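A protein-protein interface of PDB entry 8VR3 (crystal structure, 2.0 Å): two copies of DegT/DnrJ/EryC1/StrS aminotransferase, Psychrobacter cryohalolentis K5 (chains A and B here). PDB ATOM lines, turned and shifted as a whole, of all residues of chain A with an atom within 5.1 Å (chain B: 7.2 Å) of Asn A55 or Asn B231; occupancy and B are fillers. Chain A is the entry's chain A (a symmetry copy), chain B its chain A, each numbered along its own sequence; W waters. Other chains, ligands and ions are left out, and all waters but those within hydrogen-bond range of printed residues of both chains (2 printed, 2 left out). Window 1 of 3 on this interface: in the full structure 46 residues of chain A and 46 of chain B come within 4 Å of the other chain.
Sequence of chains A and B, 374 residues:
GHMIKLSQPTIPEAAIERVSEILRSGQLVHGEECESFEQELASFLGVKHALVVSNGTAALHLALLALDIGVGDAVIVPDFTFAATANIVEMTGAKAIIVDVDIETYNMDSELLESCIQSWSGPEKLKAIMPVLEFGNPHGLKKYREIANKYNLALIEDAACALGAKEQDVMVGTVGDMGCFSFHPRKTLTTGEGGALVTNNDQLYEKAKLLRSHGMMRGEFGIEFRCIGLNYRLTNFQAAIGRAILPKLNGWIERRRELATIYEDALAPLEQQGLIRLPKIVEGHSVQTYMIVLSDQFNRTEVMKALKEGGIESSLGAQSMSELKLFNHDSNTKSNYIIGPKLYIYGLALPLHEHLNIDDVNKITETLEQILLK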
ATOM      1  N   VAL A  53       6.399  24.238   7.762  1.00  0.00           N
ATOM      2  CA  VAL A  53       6.545  25.487   7.033  1.00  0.00           C
ATOM      3  C   VAL A  53       6.931  25.173   5.578  1.00  0.00           C
ATOM      4  O   VAL A  53       7.193  24.022   5.206  1.00  0.00           O
ATOM      5  CB  VAL A  53       7.577  26.418   7.731  1.00  0.00           C
ATOM      6  CG1 VAL A  53       7.120  26.919   9.083  1.00  0.00           C
ATOM      7  CG2 VAL A  53       8.932  25.747   7.896  1.00  0.00           C
ATOM      8  N   SER A  54       6.998  26.239   4.778  1.00  0.00           N
ATOM      9  CA  SER A  54       7.193  26.199   3.337  1.00  0.00           C
ATOM     10  C   SER A  54       8.466  25.452   2.933  1.00  0.00           C
ATOM     11  O   SER A  54       8.443  24.769   1.936  1.00  0.00           O
ATOM     12  CB  SER A  54       7.227  27.619   2.794  1.00  0.00           C
ATOM     13  OG  SER A  54       5.951  28.221   2.873  1.00  0.00           O
ATOM     14  N   ASN A  55       9.564  25.627   3.681  1.00  0.00           N
ATOM     15  CA  ASN A  55      10.887  25.141   3.317  1.00  0.00           C
ATOM     16  C   ASN A  55      11.830  25.342   4.508  1.00  0.00           C
ATOM     17  O   ASN A  55      11.489  26.000   5.485  1.00  0.00           O
ATOM     18  CB  ASN A  55      11.409  25.808   2.035  1.00  0.00           C
ATOM     19  CG  ASN A  55      11.417  27.327   2.086  1.00  0.00           C
ATOM     20  OD1 ASN A  55      12.113  27.933   2.900  1.00  0.00           O
ATOM     21  ND2 ASN A  55      10.598  27.959   1.245  1.00  0.00           N
ATOM     22  N   GLY A  56      13.009  24.706   4.457  1.00  0.00           N
ATOM     23  CA  GLY A  56      13.966  24.773   5.556  1.00  0.00           C
ATOM     24  C   GLY A  56      14.512  26.199   5.771  1.00  0.00           C
ATOM     25  O   GLY A  56      14.846  26.590   6.886  1.00  0.00           O
ATOM     26  N   THR A  57      14.630  26.975   4.699  1.00  0.00           N
ATOM     27  CA  THR A  57      15.010  28.379   4.815  1.00  0.00           C
ATOM     28  C   THR A  57      13.990  29.132   5.676  1.00  0.00           C
ATOM     29  O   THR A  57      14.372  29.910   6.565  1.00  0.00           O
ATOM     30  CB  THR A  57      15.243  28.989   3.429  1.00  0.00           C
ATOM     31  OG1 THR A  57      16.240  28.235   2.736  1.00  0.00           O
ATOM     32  CG2 THR A  57      15.632  30.451   3.465  1.00  0.00           C
ATOM     33  N   ALA A  58      12.697  28.891   5.440  1.00  0.00           N
ATOM     34  CA  ALA A  58      11.634  29.563   6.186  1.00  0.00           C
ATOM     35  C   ALA A  58      11.693  29.224   7.681  1.00  0.00           C
ATOM     36  O   ALA A  58      11.389  30.064   8.520  1.00  0.00           O
ATOM     37  CB  ALA A  58      10.291  29.182   5.608  1.00  0.00           C
ATOM     38  N   ALA A  59      12.097  27.992   8.008  1.00  0.00           N
ATOM     39  CA  ALA A  59      12.270  27.565   9.383  1.00  0.00           C
ATOM     40  C   ALA A  59      13.391  28.381  10.030  1.00  0.00           C
ATOM     41  O   ALA A  59      13.167  28.964  11.088  1.00  0.00           O
ATOM     42  CB  ALA A  59      12.470  26.055   9.472  1.00  0.00           C
ATOM     43  N   PHE A 181      14.552  22.028  10.127  1.00  0.00           N
ATOM     44  CA  PHE A 181      14.729  20.932   9.188  1.00  0.00           C
ATOM     45  C   PHE A 181      14.267  21.366   7.803  1.00  0.00           C
ATOM     46  O   PHE A 181      13.390  22.212   7.737  1.00  0.00           O
ATOM     47  CB  PHE A 181      13.965  19.691   9.640  1.00  0.00           C
ATOM     48  CG  PHE A 181      14.368  19.185  11.003  1.00  0.00           C
ATOM     49  CD1 PHE A 181      13.637  19.532  12.130  1.00  0.00           C
ATOM     50  CD2 PHE A 181      15.480  18.373  11.158  1.00  0.00           C
ATOM     51  CE1 PHE A 181      13.986  19.054  13.386  1.00  0.00           C
ATOM     52  CE2 PHE A 181      15.832  17.902  12.413  1.00  0.00           C
ATOM     53  CZ  PHE A 181      15.092  18.250  13.530  1.00  0.00           C
ATOM     54  N1  LLP A 187      20.618  24.722   5.381  1.00  0.00           N
ATOM     55  C2  LLP A 187      21.263  23.670   4.866  1.00  0.00           C
ATOM     56  C2' LLP A 187      22.466  23.179   5.592  1.00  0.00           C
ATOM     57  C3  LLP A 187      20.763  22.983   3.727  1.00  0.00           C
ATOM     58  O3  LLP A 187      21.352  21.899   3.159  1.00  0.00           O
ATOM     59  C4  LLP A 187      19.606  23.431   3.066  1.00  0.00           C
ATOM     60  C4' LLP A 187      19.068  22.691   1.857  1.00  0.00           C
ATOM     61  C5  LLP A 187      18.980  24.572   3.622  1.00  0.00           C
ATOM     62  C6  LLP A 187      19.512  25.161   4.744  1.00  0.00           C
ATOM     63  C5' LLP A 187      17.764  25.225   3.021  1.00  0.00           C
ATOM     64  OP4 LLP A 187      16.558  24.416   3.021  1.00  0.00           O
ATOM     65  P   LLP A 187      15.447  24.513   1.861  1.00  0.00           P
ATOM     66  OP1 LLP A 187      14.467  23.495   2.422  1.00  0.00           O
ATOM     67  OP2 LLP A 187      15.010  25.947   1.830  1.00  0.00           O
ATOM     68  OP3 LLP A 187      16.122  24.062   0.579  1.00  0.00           O
ATOM     69  N   LLP A 187      16.846  15.797   0.551  1.00  0.00           N
ATOM     70  CA  LLP A 187      16.873  15.524   1.976  1.00  0.00           C
ATOM     71  CB  LLP A 187      16.530  16.851   2.705  1.00  0.00           C
ATOM     72  CG  LLP A 187      17.700  17.837   3.039  1.00  0.00           C
ATOM     73  CD  LLP A 187      18.193  18.902   2.031  1.00  0.00           C
ATOM     74  CE  LLP A 187      19.021  20.184   2.580  1.00  0.00           C
ATOM     75  NZ  LLP A 187      19.038  21.321   1.605  1.00  0.00           N
ATOM     76  C   LLP A 187      16.069  14.211   2.054  1.00  0.00           C
ATOM     77  O   LLP A 187      15.469  13.795   1.071  1.00  0.00           O
ATOM     78  N   GLU A 193       8.944  20.721  -1.532  1.00  0.00           N
ATOM     79  CA  GLU A 193       9.494  21.731  -0.657  1.00  0.00           C
ATOM     80  C   GLU A 193       8.749  21.653   0.672  1.00  0.00           C
ATOM     81  O   GLU A 193       7.559  21.403   0.721  1.00  0.00           O
ATOM     82  CB  GLU A 193       9.312  23.140  -1.214  1.00  0.00           C
ATOM     83  CG  GLU A 193      10.008  23.422  -2.530  1.00  0.00           C
ATOM     84  CD  GLU A 193      11.466  23.849  -2.477  1.00  0.00           C
ATOM     85  OE1 GLU A 193      12.036  23.996  -1.378  1.00  0.00           O
ATOM     86  OE2 GLU A 193      12.026  24.032  -3.574  1.00  0.00           O
ATOM     87  N   GLY A 194       9.459  21.921   1.760  1.00  0.00           N
ATOM     88  CA  GLY A 194       8.892  21.835   3.095  1.00  0.00           C
ATOM     89  C   GLY A 194      10.004  21.982   4.123  1.00  0.00           C
ATOM     90  O   GLY A 194      11.184  21.925   3.761  1.00  0.00           O
ATOM     91  N   GLY A 195       9.607  22.240   5.373  1.00  0.00           N
ATOM     92  CA  GLY A 195      10.542  22.397   6.475  1.00  0.00           C
ATOM     93  C   GLY A 195       9.818  22.250   7.811  1.00  0.00           C
ATOM     94  O   GLY A 195       8.610  22.072   7.826  1.00  0.00           O
ATOM     95  N   TYR A 232       4.299  31.464   5.563  1.00  0.00           N
ATOM     96  CA  TYR A 232       5.194  30.346   5.354  1.00  0.00           C
ATOM     97  C   TYR A 232       4.477  29.037   5.659  1.00  0.00           C
ATOM     98  O   TYR A 232       5.099  28.065   6.101  1.00  0.00           O
ATOM     99  CB  TYR A 232       6.416  30.478   6.273  1.00  0.00           C
ATOM    100  CG  TYR A 232       7.564  31.320   5.779  1.00  0.00           C
ATOM    101  CD1 TYR A 232       7.972  31.289   4.458  1.00  0.00           C
ATOM    102  CD2 TYR A 232       8.329  32.044   6.678  1.00  0.00           C
ATOM    103  CE1 TYR A 232       9.118  31.938   4.046  1.00  0.00           C
ATOM    104  CE2 TYR A 232       9.429  32.759   6.274  1.00  0.00           C
ATOM    105  CZ  TYR A 232       9.850  32.674   4.963  1.00  0.00           C
ATOM    106  OH  TYR A 232      10.955  33.363   4.560  1.00  0.00           O
ATOM    107  N   SER B  54       5.824  30.669  -3.615  1.00  0.00           N
ATOM    108  CA  SER B  54       5.210  29.909  -2.537  1.00  0.00           C
ATOM    109  C   SER B  54       3.751  30.301  -2.295  1.00  0.00           C
ATOM    110  O   SER B  54       2.961  29.435  -2.002  1.00  0.00           O
ATOM    111  CB  SER B  54       6.020  30.097  -1.264  1.00  0.00           C
ATOM    112  OG  SER B  54       7.273  29.452  -1.361  1.00  0.00           O
ATOM    113  N   ALA B  58       4.333  36.038  -0.630  1.00  0.00           N
ATOM    114  CA  ALA B  58       5.717  35.979  -1.099  1.00  0.00           C
ATOM    115  C   ALA B  58       5.921  36.819  -2.366  1.00  0.00           C
ATOM    116  O   ALA B  58       6.977  37.412  -2.553  1.00  0.00           O
ATOM    117  CB  ALA B  58       6.106  34.539  -1.348  1.00  0.00           C
ATOM    118  N   LEU B  62       8.603  39.880  -2.475  1.00  0.00           N
ATOM    119  CA  LEU B  62       9.647  39.925  -3.498  1.00  0.00           C
ATOM    120  C   LEU B  62       9.496  41.213  -4.296  1.00  0.00           C
ATOM    121  O   LEU B  62      10.484  41.803  -4.667  1.00  0.00           O
ATOM    122  CB  LEU B  62       9.564  38.678  -4.397  1.00  0.00           C
ATOM    123  CG  LEU B  62      10.001  37.378  -3.718  1.00  0.00           C
ATOM    124  CD1 LEU B  62       9.708  36.162  -4.576  1.00  0.00           C
ATOM    125  CD2 LEU B  62      11.463  37.408  -3.319  1.00  0.00           C
ATOM    126  N   LEU B 211      16.148  36.692  -5.604  1.00  0.00           N
ATOM    127  CA  LEU B 211      15.602  36.692  -4.242  1.00  0.00           C
ATOM    128  C   LEU B 211      14.749  35.457  -3.945  1.00  0.00           C
ATOM    129  O   LEU B 211      14.824  34.955  -2.823  1.00  0.00           O
ATOM    130  CB  LEU B 211      14.824  37.984  -4.020  1.00  0.00           C
ATOM    131  CG  LEU B 211      15.673  39.260  -4.011  1.00  0.00           C
ATOM    132  CD1 LEU B 211      14.807  40.486  -4.015  1.00  0.00           C
ATOM    133  CD2 LEU B 211      16.620  39.334  -2.820  1.00  0.00           C
ATOM    134  N   ARG B 212      14.032  34.937  -4.963  1.00  0.00           N
ATOM    135  CA  ARG B 212      13.176  33.764  -4.829  1.00  0.00           C
ATOM    136  C   ARG B 212      13.960  32.498  -4.468  1.00  0.00           C
ATOM    137  O   ARG B 212      13.401  31.554  -3.890  1.00  0.00           O
ATOM    138  CB  ARG B 212      12.422  33.496  -6.128  1.00  0.00           C
ATOM    139  CG  ARG B 212      11.472  32.308  -6.052  1.00  0.00           C
ATOM    140  CD  ARG B 212      10.781  32.017  -7.367  1.00  0.00           C
ATOM    141  NE  ARG B 212      11.658  31.646  -8.461  1.00  0.00           N
ATOM    142  CZ  ARG B 212      11.256  31.381  -9.693  1.00  0.00           C
ATOM    143  NH1 ARG B 212       9.973  31.463  -9.999  1.00  0.00           N
ATOM    144  NH2 ARG B 212      12.139  31.031 -10.618  1.00  0.00           N
ATOM    145  N   SER B 213      15.252  32.416  -4.838  1.00  0.00           N
ATOM    146  CA  SER B 213      15.968  31.180  -4.616  1.00  0.00           C
ATOM    147  C   SER B 213      17.447  31.407  -4.296  1.00  0.00           C
ATOM    148  O   SER B 213      18.319  31.016  -5.078  1.00  0.00           O
ATOM    149  CB  SER B 213      15.788  30.306  -5.821  1.00  0.00           C
ATOM    150  OG  SER B 213      16.426  29.068  -5.544  1.00  0.00           O
ATOM    151  N   HIS B 214      17.735  32.076  -3.171  1.00  0.00           N
ATOM    152  CA  HIS B 214      19.069  32.062  -2.598  1.00  0.00           C
ATOM    153  C   HIS B 214      20.107  32.738  -3.491  1.00  0.00           C
ATOM    154  O   HIS B 214      21.286  32.432  -3.412  1.00  0.00           O
ATOM    155  CB  HIS B 214      19.560  30.626  -2.409  1.00  0.00           C
ATOM    156  CG  HIS B 214      18.615  29.752  -1.645  1.00  0.00           C
ATOM    157  ND1 HIS B 214      18.253  29.992  -0.330  1.00  0.00           N
ATOM    158  CD2 HIS B 214      17.963  28.622  -2.037  1.00  0.00           C
ATOM    159  CE1 HIS B 214      17.405  29.039   0.047  1.00  0.00           C
ATOM    160  NE2 HIS B 214      17.226  28.171  -0.965  1.00  0.00           N
ATOM    161  N   GLY B 229      19.575  35.846  -0.793  1.00  0.00           N
ATOM    162  CA  GLY B 229      18.162  35.671  -1.082  1.00  0.00           C
ATOM    163  C   GLY B 229      17.457  34.788  -0.063  1.00  0.00           C
ATOM    164  O   GLY B 229      18.024  34.456   0.978  1.00  0.00           O
ATOM    165  N   LEU B 230      16.223  34.423  -0.428  1.00  0.00           N
ATOM    166  CA  LEU B 230      15.280  33.651   0.370  1.00  0.00           C
ATOM    167  C   LEU B 230      14.997  32.342  -0.352  1.00  0.00           C
ATOM    168  O   LEU B 230      15.554  32.085  -1.416  1.00  0.00           O
ATOM    169  CB  LEU B 230      13.967  34.447   0.455  1.00  0.00           C
ATOM    170  CG  LEU B 230      14.030  35.728   1.268  1.00  0.00           C
ATOM    171  CD1 LEU B 230      12.790  36.558   1.028  1.00  0.00           C
ATOM    172  CD2 LEU B 230      14.154  35.402   2.732  1.00  0.00           C
ATOM    173  N   ASN B 231      14.040  31.566   0.184  1.00  0.00           N
ATOM    174  CA  ASN B 231      13.451  30.475  -0.569  1.00  0.00           C
ATOM    175  C   ASN B 231      11.949  30.701  -0.655  1.00  0.00           C
ATOM    176  O   ASN B 231      11.240  30.524   0.332  1.00  0.00           O
ATOM    177  CB  ASN B 231      13.799  29.119   0.036  1.00  0.00           C
ATOM    178  CG  ASN B 231      13.232  27.959  -0.743  1.00  0.00           C
ATOM    179  OD1 ASN B 231      12.522  28.148  -1.727  1.00  0.00           O
ATOM    180  ND2 ASN B 231      13.530  26.743  -0.312  1.00  0.00           N
ATOM    181  N   TYR B 232      11.473  31.068  -1.844  1.00  0.00           N
ATOM    182  CA  TYR B 232      10.051  31.182  -2.091  1.00  0.00           C
ATOM    183  C   TYR B 232       9.673  30.403  -3.344  1.00  0.00           C
ATOM    184  O   TYR B 232       8.737  30.775  -4.060  1.00  0.00           O
ATOM    185  CB  TYR B 232       9.673  32.657  -2.279  1.00  0.00           C
ATOM    186  CG  TYR B 232       9.389  33.461  -1.037  1.00  0.00           C
ATOM    187  CD1 TYR B 232       8.685  32.929   0.028  1.00  0.00           C
ATOM    188  CD2 TYR B 232       9.710  34.807  -0.995  1.00  0.00           C
ATOM    189  CE1 TYR B 232       8.291  33.714   1.092  1.00  0.00           C
ATOM    190  CE2 TYR B 232       9.394  35.588   0.089  1.00  0.00           C
ATOM    191  CZ  TYR B 232       8.648  35.053   1.118  1.00  0.00           C
ATOM    192  OH  TYR B 232       8.311  35.829   2.187  1.00  0.00           O
ATOM    193  N   ARG B 233      10.336  29.272  -3.558  1.00  0.00           N
ATOM    194  CA  ARG B 233      10.071  28.440  -4.710  1.00  0.00           C
ATOM    195  C   ARG B 233       8.741  27.704  -4.538  1.00  0.00           C
ATOM    196  O   ARG B 233       8.360  27.300  -3.442  1.00  0.00           O
ATOM    197  CB  ARG B 233      11.181  27.396  -4.909  1.00  0.00           C
ATOM    198  CG  ARG B 233      12.563  27.935  -5.259  1.00  0.00           C
ATOM    199  CD  ARG B 233      13.499  26.830  -5.748  1.00  0.00           C
ATOM    200  NE  ARG B 233      13.803  25.820  -4.714  1.00  0.00           N
ATOM    201  CZ  ARG B 233      14.789  25.903  -3.815  1.00  0.00           C
ATOM    202  NH1 ARG B 233      15.492  27.022  -3.756  1.00  0.00           N
ATOM    203  NH2 ARG B 233      15.077  24.889  -2.993  1.00  0.00           N
ATOM    204  N   LEU B 234       8.073  27.447  -5.663  1.00  0.00           N
ATOM    205  CA  LEU B 234       6.871  26.623  -5.701  1.00  0.00           C
ATOM    206  C   LEU B 234       7.281  25.237  -6.174  1.00  0.00           C
ATOM    207  O   LEU B 234       8.153  25.152  -7.027  1.00  0.00           O
ATOM    208  CB  LEU B 234       5.910  27.274  -6.695  1.00  0.00           C
ATOM    209  CG  LEU B 234       4.524  26.638  -6.775  1.00  0.00           C
ATOM    210  CD1 LEU B 234       3.747  26.864  -5.498  1.00  0.00           C
ATOM    211  CD2 LEU B 234       3.758  27.166  -7.977  1.00  0.00           C
HETATM  212  O   HOH W   1      12.509  31.735   2.672  1.00  0.00           O
HETATM  213  O   HOH W   2      10.627  23.917  -5.777  1.00  0.00           O
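Water W2 bridges OE2 of Glu A193 (2.6 Å) and O of Leu B234 (3.0 Å). Water W1 lies within hydrogen-bond range of the backbone carbonyl oxygen (O) of Asn B231 (2.9 Å) and the side-chain hydroxyl (OH) of Tyr A232 (2.9 Å).
The backbone carbonyl oxygen of Asn B231 sits at hydrogen-bond distance from the side-chain amide nitrogen of Asn A55 (2.8 Å). OP2 of LLP A187 is in hydrogen-bond range of the side-chain amide nitrogen (ND2) of Asn B231 (2.7 Å). The side-chain carboxylate (OE1) of Glu A193 lies within hydrogen-bond range of the side-chain amide nitrogen (ND2) of Asn B231 (3.3 Å). The guanidinium group of Arg B233 lies close to OP3 of LLP A187. The guanidinium group of Arg B233 is in salt-bridge range of the side-chain carboxylate of Glu A193 (2.8 Å).
Tyr B232 touches its own counterpart, Tyr A232. Positions printed for both chains: 54, 58 and 232.
Of the 13 printed residues of chain A, 5 touch a printed residue of chain B. Printed residues of chain A that touch a printed residue of chain B: Asn A55, Thr A57, LLP A187, Glu A193 and Tyr A232. Of the 13 printed residues of chain B, 4 touch a printed residue of chain A. Printed residues of chain B that touch a printed residue of chain A: His B214, Asn B231, Tyr B232 and Arg B233.
Asn A55 touches one residue of chain B. Phe A181 touches none of the printed residues of chain B. Printed residues of chain B within 4 Å of LLP A187: Asn B231 and Arg B233. Printed residues of chain B within 4 Å of Glu A193: Asn B231 (3.3 Å) and Arg B233 (2.8 Å). Printed residues of chain B within 4 Å of Tyr A232: Tyr B232. Of chain A, only Asn A55 (2.8 Å), Thr A57 (3.7 Å), LLP A187 (2.7 Å) and Glu A193 (3.3 Å) come within 4 Å of Asn B231. Printed residues of chain A within 4 Å of Tyr B232: Tyr A232. Of the printed residues of chain A, Arg B233 touches LLP A187 (3.8 Å) and Glu A193 (2.8 Å).
Thr A57 touches His B214 (OG1 to CE1, 3.0 Å). CB of Thr A57 touches CB of Asn B231 (3.7 Å). Tyr B232 touches Tyr A232 (CE1 to CE1, 3.5 Å).
The backbone NH (N) of Ser B54 is in hydrogen-bond range of the backbone carbonyl oxygen (O) of Tyr B232, at 2.9 Å. OG of Ser B54 lies within hydrogen-bond range of O of Arg B233. N of Tyr B232 lies within hydrogen-bond range of O of Arg B212 (2.9 Å). A ring nitrogen (NE2) of His B214 sits close to the guanidinium group (NH1) of Arg B233 (3.5 Å). The side-chain amide oxygen (OD1) of Asn A55 sits at hydrogen-bond distance from the backbone NH (N) of Ala A58. OP2 of LLP A187 sits at hydrogen-bond distance from the side-chain hydroxyl (OG1) of Thr A57, 2.8 Å away.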
